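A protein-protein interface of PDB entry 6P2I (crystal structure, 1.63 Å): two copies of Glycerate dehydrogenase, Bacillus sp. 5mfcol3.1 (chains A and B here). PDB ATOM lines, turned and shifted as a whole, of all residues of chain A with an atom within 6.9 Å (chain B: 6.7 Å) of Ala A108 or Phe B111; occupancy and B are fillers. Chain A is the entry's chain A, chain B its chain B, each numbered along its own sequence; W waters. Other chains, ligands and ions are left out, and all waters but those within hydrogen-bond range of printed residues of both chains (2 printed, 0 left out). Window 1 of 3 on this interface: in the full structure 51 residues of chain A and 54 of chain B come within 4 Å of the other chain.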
ATOM      1  N   VAL A 102      24.938 -14.990 -28.930  1.00  0.00           N
ATOM      2  CA  VAL A 102      24.435 -14.895 -30.297  1.00  0.00           C
ATOM      3  C   VAL A 102      23.610 -16.128 -30.642  1.00  0.00           C
ATOM      4  O   VAL A 102      22.555 -16.025 -31.278  1.00  0.00           O
ATOM      5  CB  VAL A 102      25.588 -14.689 -31.297  1.00  0.00           C
ATOM      6  CG1 VAL A 102      25.059 -14.675 -32.735  1.00  0.00           C
ATOM      7  CG2 VAL A 102      26.301 -13.370 -30.987  1.00  0.00           C
ATOM      8  N   ALA A 103      24.081 -17.311 -30.238  1.00  0.00           N
ATOM      9  CA  ALA A 103      23.313 -18.523 -30.502  1.00  0.00           C
ATOM     10  C   ALA A 103      21.929 -18.449 -29.866  1.00  0.00           C
ATOM     11  O   ALA A 103      20.929 -18.819 -30.497  1.00  0.00           O
ATOM     12  CB  ALA A 103      24.076 -19.747 -29.996  1.00  0.00           C
ATOM     13  N   GLU A 104      21.841 -17.961 -28.628  1.00  0.00           N
ATOM     14  CA  GLU A 104      20.517 -17.804 -28.028  1.00  0.00           C
ATOM     15  C   GLU A 104      19.690 -16.773 -28.781  1.00  0.00           C
ATOM     16  O   GLU A 104      18.471 -16.933 -28.922  1.00  0.00           O
ATOM     17  CB  GLU A 104      20.639 -17.431 -26.549  1.00  0.00           C
ATOM     18  CG  GLU A 104      21.137 -18.587 -25.711  1.00  0.00           C
ATOM     19  CD  GLU A 104      21.138 -18.326 -24.214  1.00  0.00           C
ATOM     20  OE1 GLU A 104      20.443 -17.394 -23.753  1.00  0.00           O
ATOM     21  OE2 GLU A 104      21.849 -19.072 -23.500  1.00  0.00           O
ATOM     22  N   HIS A 105      20.338 -15.723 -29.302  1.00  0.00           N
ATOM     23  CA  HIS A 105      19.602 -14.724 -30.064  1.00  0.00           C
ATOM     24  C   HIS A 105      19.021 -15.297 -31.339  1.00  0.00           C
ATOM     25  O   HIS A 105      17.962 -14.841 -31.793  1.00  0.00           O
ATOM     26  CB  HIS A 105      20.520 -13.546 -30.404  1.00  0.00           C
ATOM     27  CG  HIS A 105      19.790 -12.285 -30.707  1.00  0.00           C
ATOM     28  ND1 HIS A 105      19.252 -11.483 -29.722  1.00  0.00           N
ATOM     29  CD2 HIS A 105      19.540 -11.658 -31.883  1.00  0.00           C
ATOM     30  CE1 HIS A 105      18.711 -10.413 -30.279  1.00  0.00           C
ATOM     31  NE2 HIS A 105      18.864 -10.499 -31.588  1.00  0.00           N
ATOM     32  N   VAL A 106      19.702 -16.269 -31.956  1.00  0.00           N
ATOM     33  CA  VAL A 106      19.137 -16.909 -33.137  1.00  0.00           C
ATOM     34  C   VAL A 106      17.766 -17.491 -32.805  1.00  0.00           C
ATOM     35  O   VAL A 106      16.803 -17.334 -33.569  1.00  0.00           O
ATOM     36  CB  VAL A 106      20.083 -18.006 -33.665  1.00  0.00           C
ATOM     37  CG1 VAL A 106      19.384 -18.870 -34.707  1.00  0.00           C
ATOM     38  CG2 VAL A 106      21.367 -17.397 -34.250  1.00  0.00           C
ATOM     39  N   PHE A 107      17.659 -18.148 -31.654  1.00  0.00           N
ATOM     40  CA  PHE A 107      16.379 -18.733 -31.266  1.00  0.00           C
ATOM     41  C   PHE A 107      15.398 -17.666 -30.806  1.00  0.00           C
ATOM     42  O   PHE A 107      14.203 -17.787 -31.073  1.00  0.00           O
ATOM     43  CB  PHE A 107      16.601 -19.814 -30.204  1.00  0.00           C
ATOM     44  CG  PHE A 107      17.206 -21.054 -30.776  1.00  0.00           C
ATOM     45  CD1 PHE A 107      18.583 -21.169 -30.934  1.00  0.00           C
ATOM     46  CD2 PHE A 107      16.389 -22.076 -31.224  1.00  0.00           C
ATOM     47  CE1 PHE A 107      19.132 -22.293 -31.503  1.00  0.00           C
ATOM     48  CE2 PHE A 107      16.936 -23.215 -31.796  1.00  0.00           C
ATOM     49  CZ  PHE A 107      18.302 -23.329 -31.930  1.00  0.00           C
ATOM     50  N   ALA A 108      15.879 -16.597 -30.164  1.00  0.00           N
ATOM     51  CA  ALA A 108      15.006 -15.465 -29.864  1.00  0.00           C
ATOM     52  C   ALA A 108      14.356 -14.931 -31.134  1.00  0.00           C
ATOM     53  O   ALA A 108      13.137 -14.730 -31.192  1.00  0.00           O
ATOM     54  CB  ALA A 108      15.796 -14.354 -29.158  1.00  0.00           C
ATOM     55  N   LEU A 109      15.160 -14.706 -32.178  1.00  0.00           N
ATOM     56  CA  LEU A 109      14.621 -14.189 -33.429  1.00  0.00           C
ATOM     57  C   LEU A 109      13.714 -15.200 -34.116  1.00  0.00           C
ATOM     58  O   LEU A 109      12.646 -14.835 -34.620  1.00  0.00           O
ATOM     59  CB  LEU A 109      15.761 -13.807 -34.366  1.00  0.00           C
ATOM     60  CG  LEU A 109      16.533 -12.562 -33.964  1.00  0.00           C
ATOM     61  CD1 LEU A 109      17.778 -12.424 -34.854  1.00  0.00           C
ATOM     62  CD2 LEU A 109      15.650 -11.316 -34.065  1.00  0.00           C
ATOM     63  N   LEU A 110      14.138 -16.464 -34.167  1.00  0.00           N
ATOM     64  CA  LEU A 110      13.355 -17.503 -34.825  1.00  0.00           C
ATOM     65  C   LEU A 110      11.970 -17.617 -34.207  1.00  0.00           C
ATOM     66  O   LEU A 110      10.966 -17.667 -34.919  1.00  0.00           O
ATOM     67  CB  LEU A 110      14.100 -18.842 -34.741  1.00  0.00           C
ATOM     68  CG  LEU A 110      13.355 -20.124 -35.126  1.00  0.00           C
ATOM     69  CD1 LEU A 110      12.844 -20.070 -36.560  1.00  0.00           C
ATOM     70  CD2 LEU A 110      14.271 -21.332 -34.929  1.00  0.00           C
ATOM     71  N   PHE A 111      11.906 -17.649 -32.876  1.00  0.00           N
ATOM     72  CA  PHE A 111      10.615 -17.741 -32.201  1.00  0.00           C
ATOM     73  C   PHE A 111       9.796 -16.466 -32.392  1.00  0.00           C
ATOM     74  O   PHE A 111       8.581 -16.530 -32.586  1.00  0.00           O
ATOM     75  CB  PHE A 111      10.830 -18.023 -30.712  1.00  0.00           C
ATOM     76  CG  PHE A 111      11.135 -19.468 -30.390  1.00  0.00           C
ATOM     77  CD1 PHE A 111      10.349 -20.504 -30.905  1.00  0.00           C
ATOM     78  CD2 PHE A 111      12.204 -19.790 -29.561  1.00  0.00           C
ATOM     79  CE1 PHE A 111      10.646 -21.838 -30.600  1.00  0.00           C
ATOM     80  CE2 PHE A 111      12.507 -21.097 -29.261  1.00  0.00           C
ATOM     81  CZ  PHE A 111      11.716 -22.128 -29.767  1.00  0.00           C
ATOM     82  N   ALA A 112      10.447 -15.294 -32.351  1.00  0.00           N
ATOM     83  CA  ALA A 112       9.726 -14.042 -32.561  1.00  0.00           C
ATOM     84  C   ALA A 112       9.088 -14.004 -33.945  1.00  0.00           C
ATOM     85  O   ALA A 112       7.962 -13.521 -34.108  1.00  0.00           O
ATOM     86  CB  ALA A 112      10.678 -12.856 -32.365  1.00  0.00           C
ATOM     87  N   VAL A 113       9.792 -14.516 -34.959  1.00  0.00           N
ATOM     88  CA  VAL A 113       9.209 -14.609 -36.296  1.00  0.00           C
ATOM     89  C   VAL A 113       8.105 -15.656 -36.318  1.00  0.00           C
ATOM     90  O   VAL A 113       6.984 -15.395 -36.779  1.00  0.00           O
ATOM     91  CB  VAL A 113      10.295 -14.944 -37.334  1.00  0.00           C
ATOM     92  CG1 VAL A 113       9.667 -15.236 -38.698  1.00  0.00           C
ATOM     93  CG2 VAL A 113      11.327 -13.807 -37.448  1.00  0.00           C
ATOM     94  N   ILE A 117       5.426 -12.574 -32.596  1.00  0.00           N
ATOM     95  CA  ILE A 117       5.363 -11.939 -31.280  1.00  0.00           C
ATOM     96  C   ILE A 117       4.974 -10.467 -31.390  1.00  0.00           C
ATOM     97  O   ILE A 117       4.209  -9.955 -30.564  1.00  0.00           O
ATOM     98  CB  ILE A 117       6.706 -12.118 -30.546  1.00  0.00           C
ATOM     99  CG1 ILE A 117       6.917 -13.594 -30.172  1.00  0.00           C
ATOM    100  CG2 ILE A 117       6.761 -11.242 -29.299  1.00  0.00           C
ATOM    101  CD1 ILE A 117       5.960 -14.105 -29.071  1.00  0.00           C
ATOM    102  N   ILE A 160      22.249 -26.311 -29.557  1.00  0.00           N
ATOM    103  CA  ILE A 160      20.898 -25.993 -29.109  1.00  0.00           C
ATOM    104  C   ILE A 160      19.871 -26.655 -30.019  1.00  0.00           C
ATOM    105  O   ILE A 160      18.881 -27.232 -29.546  1.00  0.00           O
ATOM    106  CB  ILE A 160      20.691 -24.473 -29.048  1.00  0.00           C
ATOM    107  CG1 ILE A 160      21.649 -23.834 -28.034  1.00  0.00           C
ATOM    108  CG2 ILE A 160      19.244 -24.159 -28.703  1.00  0.00           C
ATOM    109  CD1 ILE A 160      21.651 -22.342 -28.099  1.00  0.00           C
ATOM    110  N   PHE A 164      16.985 -29.420 -29.206  1.00  0.00           N
ATOM    111  CA  PHE A 164      15.595 -29.195 -29.600  1.00  0.00           C
ATOM    112  C   PHE A 164      15.066 -30.320 -30.479  1.00  0.00           C
ATOM    113  O   PHE A 164      13.887 -30.286 -30.855  1.00  0.00           O
ATOM    114  CB  PHE A 164      15.449 -27.890 -30.375  1.00  0.00           C
ATOM    115  CG  PHE A 164      14.814 -26.767 -29.606  1.00  0.00           C
ATOM    116  CD1 PHE A 164      13.457 -26.746 -29.365  1.00  0.00           C
ATOM    117  CD2 PHE A 164      15.584 -25.693 -29.172  1.00  0.00           C
ATOM    118  CE1 PHE A 164      12.885 -25.700 -28.679  1.00  0.00           C
ATOM    119  CE2 PHE A 164      15.014 -24.643 -28.490  1.00  0.00           C
ATOM    120  CZ  PHE A 164      13.659 -24.645 -28.242  1.00  0.00           C
ATOM    121  N   ILE A 225      17.433 -16.239 -40.689  1.00  0.00           N
ATOM    122  CA  ILE A 225      18.003 -15.530 -39.544  1.00  0.00           C
ATOM    123  C   ILE A 225      19.377 -15.010 -39.944  1.00  0.00           C
ATOM    124  O   ILE A 225      20.200 -15.769 -40.464  1.00  0.00           O
ATOM    125  CB  ILE A 225      18.111 -16.439 -38.303  1.00  0.00           C
ATOM    126  CG1 ILE A 225      16.754 -17.082 -37.955  1.00  0.00           C
ATOM    127  CG2 ILE A 225      18.691 -15.653 -37.124  1.00  0.00           C
ATOM    128  CD1 ILE A 225      15.678 -16.067 -37.565  1.00  0.00           C
ATOM    129  N   VAL A 270      11.549  -9.382 -38.056  1.00  0.00           N
ATOM    130  CA  VAL A 270      11.856  -8.954 -36.702  1.00  0.00           C
ATOM    131  C   VAL A 270      13.282  -8.425 -36.729  1.00  0.00           C
ATOM    132  O   VAL A 270      14.194  -9.120 -37.191  1.00  0.00           O
ATOM    133  CB  VAL A 270      11.702 -10.110 -35.697  1.00  0.00           C
ATOM    134  CG1 VAL A 270      12.133  -9.697 -34.303  1.00  0.00           C
ATOM    135  CG2 VAL A 270      10.247 -10.602 -35.699  1.00  0.00           C
ATOM    136  N   VAL B 106       6.906 -21.199 -24.456  1.00  0.00           N
ATOM    137  CA  VAL B 106       7.555 -20.755 -23.228  1.00  0.00           C
ATOM    138  C   VAL B 106       8.873 -20.084 -23.563  1.00  0.00           C
ATOM    139  O   VAL B 106       9.193 -19.006 -23.047  1.00  0.00           O
ATOM    140  CB  VAL B 106       7.758 -21.934 -22.264  1.00  0.00           C
ATOM    141  CG1 VAL B 106       8.740 -21.539 -21.161  1.00  0.00           C
ATOM    142  CG2 VAL B 106       6.417 -22.354 -21.685  1.00  0.00           C
ATOM    143  N   PHE B 107       9.653 -20.714 -24.438  1.00  0.00           N
ATOM    144  CA  PHE B 107      10.940 -20.134 -24.810  1.00  0.00           C
ATOM    145  C   PHE B 107      10.772 -18.940 -25.741  1.00  0.00           C
ATOM    146  O   PHE B 107      11.566 -17.987 -25.668  1.00  0.00           O
ATOM    147  CB  PHE B 107      11.832 -21.213 -25.416  1.00  0.00           C
ATOM    148  CG  PHE B 107      12.332 -22.178 -24.385  1.00  0.00           C
ATOM    149  CD1 PHE B 107      11.541 -23.235 -23.973  1.00  0.00           C
ATOM    150  CD2 PHE B 107      13.550 -21.981 -23.769  1.00  0.00           C
ATOM    151  CE1 PHE B 107      11.981 -24.093 -22.984  1.00  0.00           C
ATOM    152  CE2 PHE B 107      13.999 -22.824 -22.796  1.00  0.00           C
ATOM    153  CZ  PHE B 107      13.205 -23.895 -22.393  1.00  0.00           C
ATOM    154  N   ALA B 108       9.740 -18.942 -26.589  1.00  0.00           N
ATOM    155  CA  ALA B 108       9.476 -17.753 -27.403  1.00  0.00           C
ATOM    156  C   ALA B 108       9.236 -16.537 -26.516  1.00  0.00           C
ATOM    157  O   ALA B 108       9.798 -15.451 -26.749  1.00  0.00           O
ATOM    158  CB  ALA B 108       8.273 -18.002 -28.321  1.00  0.00           C
ATOM    159  N   LEU B 109       8.422 -16.717 -25.471  1.00  0.00           N
ATOM    160  CA  LEU B 109       8.127 -15.643 -24.528  1.00  0.00           C
ATOM    161  C   LEU B 109       9.358 -15.281 -23.708  1.00  0.00           C
ATOM    162  O   LEU B 109       9.673 -14.093 -23.521  1.00  0.00           O
ATOM    163  CB  LEU B 109       6.976 -16.067 -23.605  1.00  0.00           C
ATOM    164  CG  LEU B 109       5.585 -16.077 -24.238  1.00  0.00           C
ATOM    165  CD1 LEU B 109       4.537 -16.707 -23.289  1.00  0.00           C
ATOM    166  CD2 LEU B 109       5.171 -14.677 -24.610  1.00  0.00           C
ATOM    167  N   LEU B 110      10.057 -16.294 -23.193  1.00  0.00           N
ATOM    168  CA  LEU B 110      11.259 -16.057 -22.403  1.00  0.00           C
ATOM    169  C   LEU B 110      12.254 -15.213 -23.182  1.00  0.00           C
ATOM    170  O   LEU B 110      12.775 -14.214 -22.674  1.00  0.00           O
ATOM    171  CB  LEU B 110      11.889 -17.394 -22.001  1.00  0.00           C
ATOM    172  CG  LEU B 110      13.264 -17.342 -21.321  1.00  0.00           C
ATOM    173  CD1 LEU B 110      13.257 -16.462 -20.066  1.00  0.00           C
ATOM    174  CD2 LEU B 110      13.726 -18.753 -20.999  1.00  0.00           C
ATOM    175  N   PHE B 111      12.527 -15.602 -24.424  1.00  0.00           N
ATOM    176  CA  PHE B 111      13.501 -14.841 -25.206  1.00  0.00           C
ATOM    177  C   PHE B 111      12.959 -13.467 -25.565  1.00  0.00           C
ATOM    178  O   PHE B 111      13.724 -12.491 -25.624  1.00  0.00           O
ATOM    179  CB  PHE B 111      13.881 -15.618 -26.462  1.00  0.00           C
ATOM    180  CG  PHE B 111      14.878 -16.708 -26.224  1.00  0.00           C
ATOM    181  CD1 PHE B 111      16.068 -16.436 -25.554  1.00  0.00           C
ATOM    182  CD2 PHE B 111      14.632 -18.011 -26.659  1.00  0.00           C
ATOM    183  CE1 PHE B 111      17.004 -17.429 -25.340  1.00  0.00           C
ATOM    184  CE2 PHE B 111      15.555 -19.017 -26.438  1.00  0.00           C
ATOM    185  CZ  PHE B 111      16.751 -18.729 -25.779  1.00  0.00           C
ATOM    186  N   ALA B 112      11.652 -13.360 -25.836  1.00  0.00           N
ATOM    187  CA  ALA B 112      11.092 -12.047 -26.161  1.00  0.00           C
ATOM    188  C   ALA B 112      11.243 -11.074 -24.997  1.00  0.00           C
ATOM    189  O   ALA B 112      11.546  -9.892 -25.201  1.00  0.00           O
ATOM    190  CB  ALA B 112       9.616 -12.180 -26.559  1.00  0.00           C
ATOM    191  N   VAL B 113      11.031 -11.552 -23.766  1.00  0.00           N
ATOM    192  CA  VAL B 113      11.252 -10.717 -22.590  1.00  0.00           C
ATOM    193  C   VAL B 113      12.738 -10.429 -22.409  1.00  0.00           C
ATOM    194  O   VAL B 113      13.145  -9.265 -22.275  1.00  0.00           O
ATOM    195  CB  VAL B 113      10.669 -11.389 -21.332  1.00  0.00           C
ATOM    196  CG1 VAL B 113      11.048 -10.579 -20.090  1.00  0.00           C
ATOM    197  CG2 VAL B 113       9.159 -11.547 -21.461  1.00  0.00           C
ATOM    198  N   ASN B 114      13.560 -11.486 -22.421  1.00  0.00           N
ATOM    199  CA  ASN B 114      14.981 -11.348 -22.103  1.00  0.00           C
ATOM    200  C   ASN B 114      15.693 -10.438 -23.092  1.00  0.00           C
ATOM    201  O   ASN B 114      16.535  -9.624 -22.693  1.00  0.00           O
ATOM    202  CB  ASN B 114      15.663 -12.717 -22.086  1.00  0.00           C
ATOM    203  CG  ASN B 114      16.071 -13.151 -20.696  1.00  0.00           C
ATOM    204  OD1 ASN B 114      15.391 -12.851 -19.711  1.00  0.00           O
ATOM    205  ND2 ASN B 114      17.181 -13.881 -20.609  1.00  0.00           N
ATOM    206  N   ARG B 115      15.379 -10.564 -24.386  1.00  0.00           N
ATOM    207  CA  ARG B 115      16.043  -9.736 -25.403  1.00  0.00           C
ATOM    208  C   ARG B 115      15.290  -8.443 -25.696  1.00  0.00           C
ATOM    209  O   ARG B 115      15.714  -7.682 -26.577  1.00  0.00           O
ATOM    210  CB  ARG B 115      16.220 -10.537 -26.710  1.00  0.00           C
ATOM    211  CG  ARG B 115      17.001 -11.850 -26.549  1.00  0.00           C
ATOM    212  CD  ARG B 115      18.346 -11.571 -25.900  1.00  0.00           C
ATOM    213  NE  ARG B 115      19.230 -12.718 -25.670  1.00  0.00           N
ATOM    214  CZ  ARG B 115      20.380 -12.915 -26.316  1.00  0.00           C
ATOM    215  NH1 ARG B 115      20.757 -12.083 -27.278  1.00  0.00           N
ATOM    216  NH2 ARG B 115      21.173 -13.927 -25.998  1.00  0.00           N
ATOM    217  N   LYS B 116      14.200  -8.168 -24.974  1.00  0.00           N
ATOM    218  CA  LYS B 116      13.378  -6.976 -25.184  1.00  0.00           C
ATOM    219  C   LYS B 116      13.063  -6.787 -26.667  1.00  0.00           C
ATOM    220  O   LYS B 116      13.228  -5.707 -27.240  1.00  0.00           O
ATOM    221  CB  LYS B 116      14.048  -5.736 -24.583  1.00  0.00           C
ATOM    222  CG  LYS B 116      14.132  -5.785 -23.056  1.00  0.00           C
ATOM    223  CD  LYS B 116      14.772  -4.501 -22.492  1.00  0.00           C
ATOM    224  CE  LYS B 116      14.921  -4.582 -20.978  1.00  0.00           C
ATOM    225  NZ  LYS B 116      15.910  -5.622 -20.547  1.00  0.00           N
ATOM    226  N   ILE B 117      12.594  -7.875 -27.288  1.00  0.00           N
ATOM    227  CA  ILE B 117      12.341  -7.899 -28.729  1.00  0.00           C
ATOM    228  C   ILE B 117      11.418  -6.765 -29.167  1.00  0.00           C
ATOM    229  O   ILE B 117      11.611  -6.164 -30.233  1.00  0.00           O
ATOM    230  CB  ILE B 117      11.761  -9.275 -29.124  1.00  0.00           C
ATOM    231  CG1 ILE B 117      12.838 -10.361 -29.027  1.00  0.00           C
ATOM    232  CG2 ILE B 117      11.105  -9.216 -30.501  1.00  0.00           C
ATOM    233  CD1 ILE B 117      13.948 -10.252 -30.082  1.00  0.00           C
ATOM    234  N   SER B 138      20.619 -11.422 -20.053  1.00  0.00           N
ATOM    235  CA  SER B 138      21.241 -12.607 -19.484  1.00  0.00           C
ATOM    236  C   SER B 138      21.100 -13.766 -20.460  1.00  0.00           C
ATOM    237  O   SER B 138      20.040 -13.953 -21.068  1.00  0.00           O
ATOM    238  CB  SER B 138      20.593 -13.006 -18.154  1.00  0.00           C
ATOM    239  OG  SER B 138      20.803 -12.044 -17.141  1.00  0.00           O
ATOM    240  N   GLU B 139      22.163 -14.551 -20.600  1.00  0.00           N
ATOM    241  CA  GLU B 139      22.010 -15.838 -21.266  1.00  0.00           C
ATOM    242  C   GLU B 139      21.191 -16.764 -20.382  1.00  0.00           C
ATOM    243  O   GLU B 139      21.282 -16.719 -19.154  1.00  0.00           O
ATOM    244  CB  GLU B 139      23.370 -16.462 -21.555  1.00  0.00           C
ATOM    245  CG  GLU B 139      24.169 -15.632 -22.543  1.00  0.00           C
ATOM    246  CD  GLU B 139      25.648 -15.928 -22.549  1.00  0.00           C
ATOM    247  OE1 GLU B 139      26.094 -16.910 -21.919  1.00  0.00           O
ATOM    248  OE2 GLU B 139      26.400 -15.124 -23.157  1.00  0.00           O
ATOM    249  N   ILE B 140      20.379 -17.609 -21.014  1.00  0.00           N
ATOM    250  CA  ILE B 140      19.566 -18.525 -20.221  1.00  0.00           C
ATOM    251  C   ILE B 140      20.322 -19.806 -19.864  1.00  0.00           C
ATOM    252  O   ILE B 140      19.942 -20.486 -18.907  1.00  0.00           O
ATOM    253  CB  ILE B 140      18.214 -18.860 -20.891  1.00  0.00           C
ATOM    254  CG1 ILE B 140      18.375 -19.797 -22.096  1.00  0.00           C
ATOM    255  CG2 ILE B 140      17.436 -17.585 -21.266  1.00  0.00           C
ATOM    256  CD1 ILE B 140      17.015 -20.387 -22.566  1.00  0.00           C
ATOM    257  N   PHE B 164      19.136 -26.290 -23.606  1.00  0.00           N
ATOM    258  CA  PHE B 164      19.912 -25.087 -23.366  1.00  0.00           C
ATOM    259  C   PHE B 164      20.898 -25.241 -22.214  1.00  0.00           C
ATOM    260  O   PHE B 164      21.614 -24.282 -21.908  1.00  0.00           O
ATOM    261  CB  PHE B 164      18.964 -23.921 -23.107  1.00  0.00           C
ATOM    262  CG  PHE B 164      18.348 -23.361 -24.355  1.00  0.00           C
ATOM    263  CD1 PHE B 164      19.024 -22.414 -25.107  1.00  0.00           C
ATOM    264  CD2 PHE B 164      17.095 -23.772 -24.775  1.00  0.00           C
ATOM    265  CE1 PHE B 164      18.468 -21.894 -26.249  1.00  0.00           C
ATOM    266  CE2 PHE B 164      16.534 -23.250 -25.927  1.00  0.00           C
ATOM    267  CZ  PHE B 164      17.219 -22.308 -26.657  1.00  0.00           C
ATOM    268  N   ILE B 225       6.767 -16.721 -16.620  1.00  0.00           N
ATOM    269  CA  ILE B 225       6.076 -17.130 -17.841  1.00  0.00           C
ATOM    270  C   ILE B 225       4.779 -17.814 -17.447  1.00  0.00           C
ATOM    271  O   ILE B 225       4.783 -18.716 -16.603  1.00  0.00           O
ATOM    272  CB  ILE B 225       6.923 -18.088 -18.702  1.00  0.00           C
ATOM    273  CG1 ILE B 225       8.280 -17.477 -19.060  1.00  0.00           C
ATOM    274  CG2 ILE B 225       6.182 -18.446 -19.985  1.00  0.00           C
ATOM    275  CD1 ILE B 225       8.180 -16.218 -19.936  1.00  0.00           C
HETATM  276  O   HOH W   1      19.394 -14.938 -23.712  1.00  0.00           O
HETATM  277  O   HOH W   2      11.089 -14.209 -29.047  1.00  0.00           O
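Water W1 lies within hydrogen-bond range of the side-chain carboxylate of Glu A104 (2.7 Å), the backbone carbonyl oxygen of Ser B138 (2.9 Å) and the guanidinium group of Arg B115 (3.0 Å). Water W2 lies within hydrogen-bond range of the backbone carbonyl oxygen of Ala B108 (2.9 Å), the backbone carbonyl oxygen of Ala A108 (3.0 Å) and the backbone NH of Ala B112 (3.4 Å).
Glu A104 touches Phe B111. Arg B115 touches Glu A104. Phe A107 touches Phe B111 (CB to CE2, 3.99 Å). Ala A108 touches Phe B111 (CB to CB, 3.5 Å). Arg B115 touches Ala A108. CE2 of Phe A111 touches CB of Phe B107, 3.9 Å away. Ala B108 touches Phe A111 (CB to CB, 3.5 Å). Ile A160 touches Phe B164. Phe B164 touches Phe A164. Val A270 touches Ile B117 (CG1 to CG2, 3.97 Å).
Hydrophobic or aromatic side chains of chain A within 4 Å of the printed part of chain B: His A105, Phe A107, Ala A108, Phe A111, Ile A160, Phe A164 and Val A270. Among the printed residues, 13 pairs touch across the chains.
Phe A107 touches Phe B111, and with the chains exchanged Phe A111 touches Phe B107. Ala A108 touches Phe B111, and with the chains exchanged Phe A111 touches Ala B108. Phe A164 touches its own counterpart, Phe B164.
Of the printed residues of chain B, Glu A104 touches Phe B111 (3.8 Å), Arg B115 (3.6 Å), Glu B139 (3.3 Å) and Ile B140 (2.7 Å). Ala A108 touches two residues of chain B. Printed residues of chain B within 4 Å of Phe A111: Phe B107 (3.9 Å) and Ala B108 (3.5 Å). Of the printed residues of chain A, Phe B111 touches Glu A104 (3.8 Å), Phe A107 (3.99 Å) and Ala A108 (3.5 Å). Val B113 touches none of the printed residues of chain A. Printed residues of chain A within 4 Å of Ile B117: Val A270 (3.97 Å). Of the printed residues of chain A, Glu B139 touches Glu A104. The nearest printed residue of chain A that does not touch Phe B107 is Phe A164 (4.8 Å).
The backbone NH of Ile B117 is in hydrogen-bond range of the backbone carbonyl oxygen of Ala B112, 3.1 Å away.
A ring nitrogen (ND1) of His A105 is in hydrogen-bond range of the guanidinium group of Arg B115, at 2.9 Å. The backbone NH of Ile B140 is in hydrogen-bond range of the side-chain carboxylate of Glu A104, 2.7 Å away.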
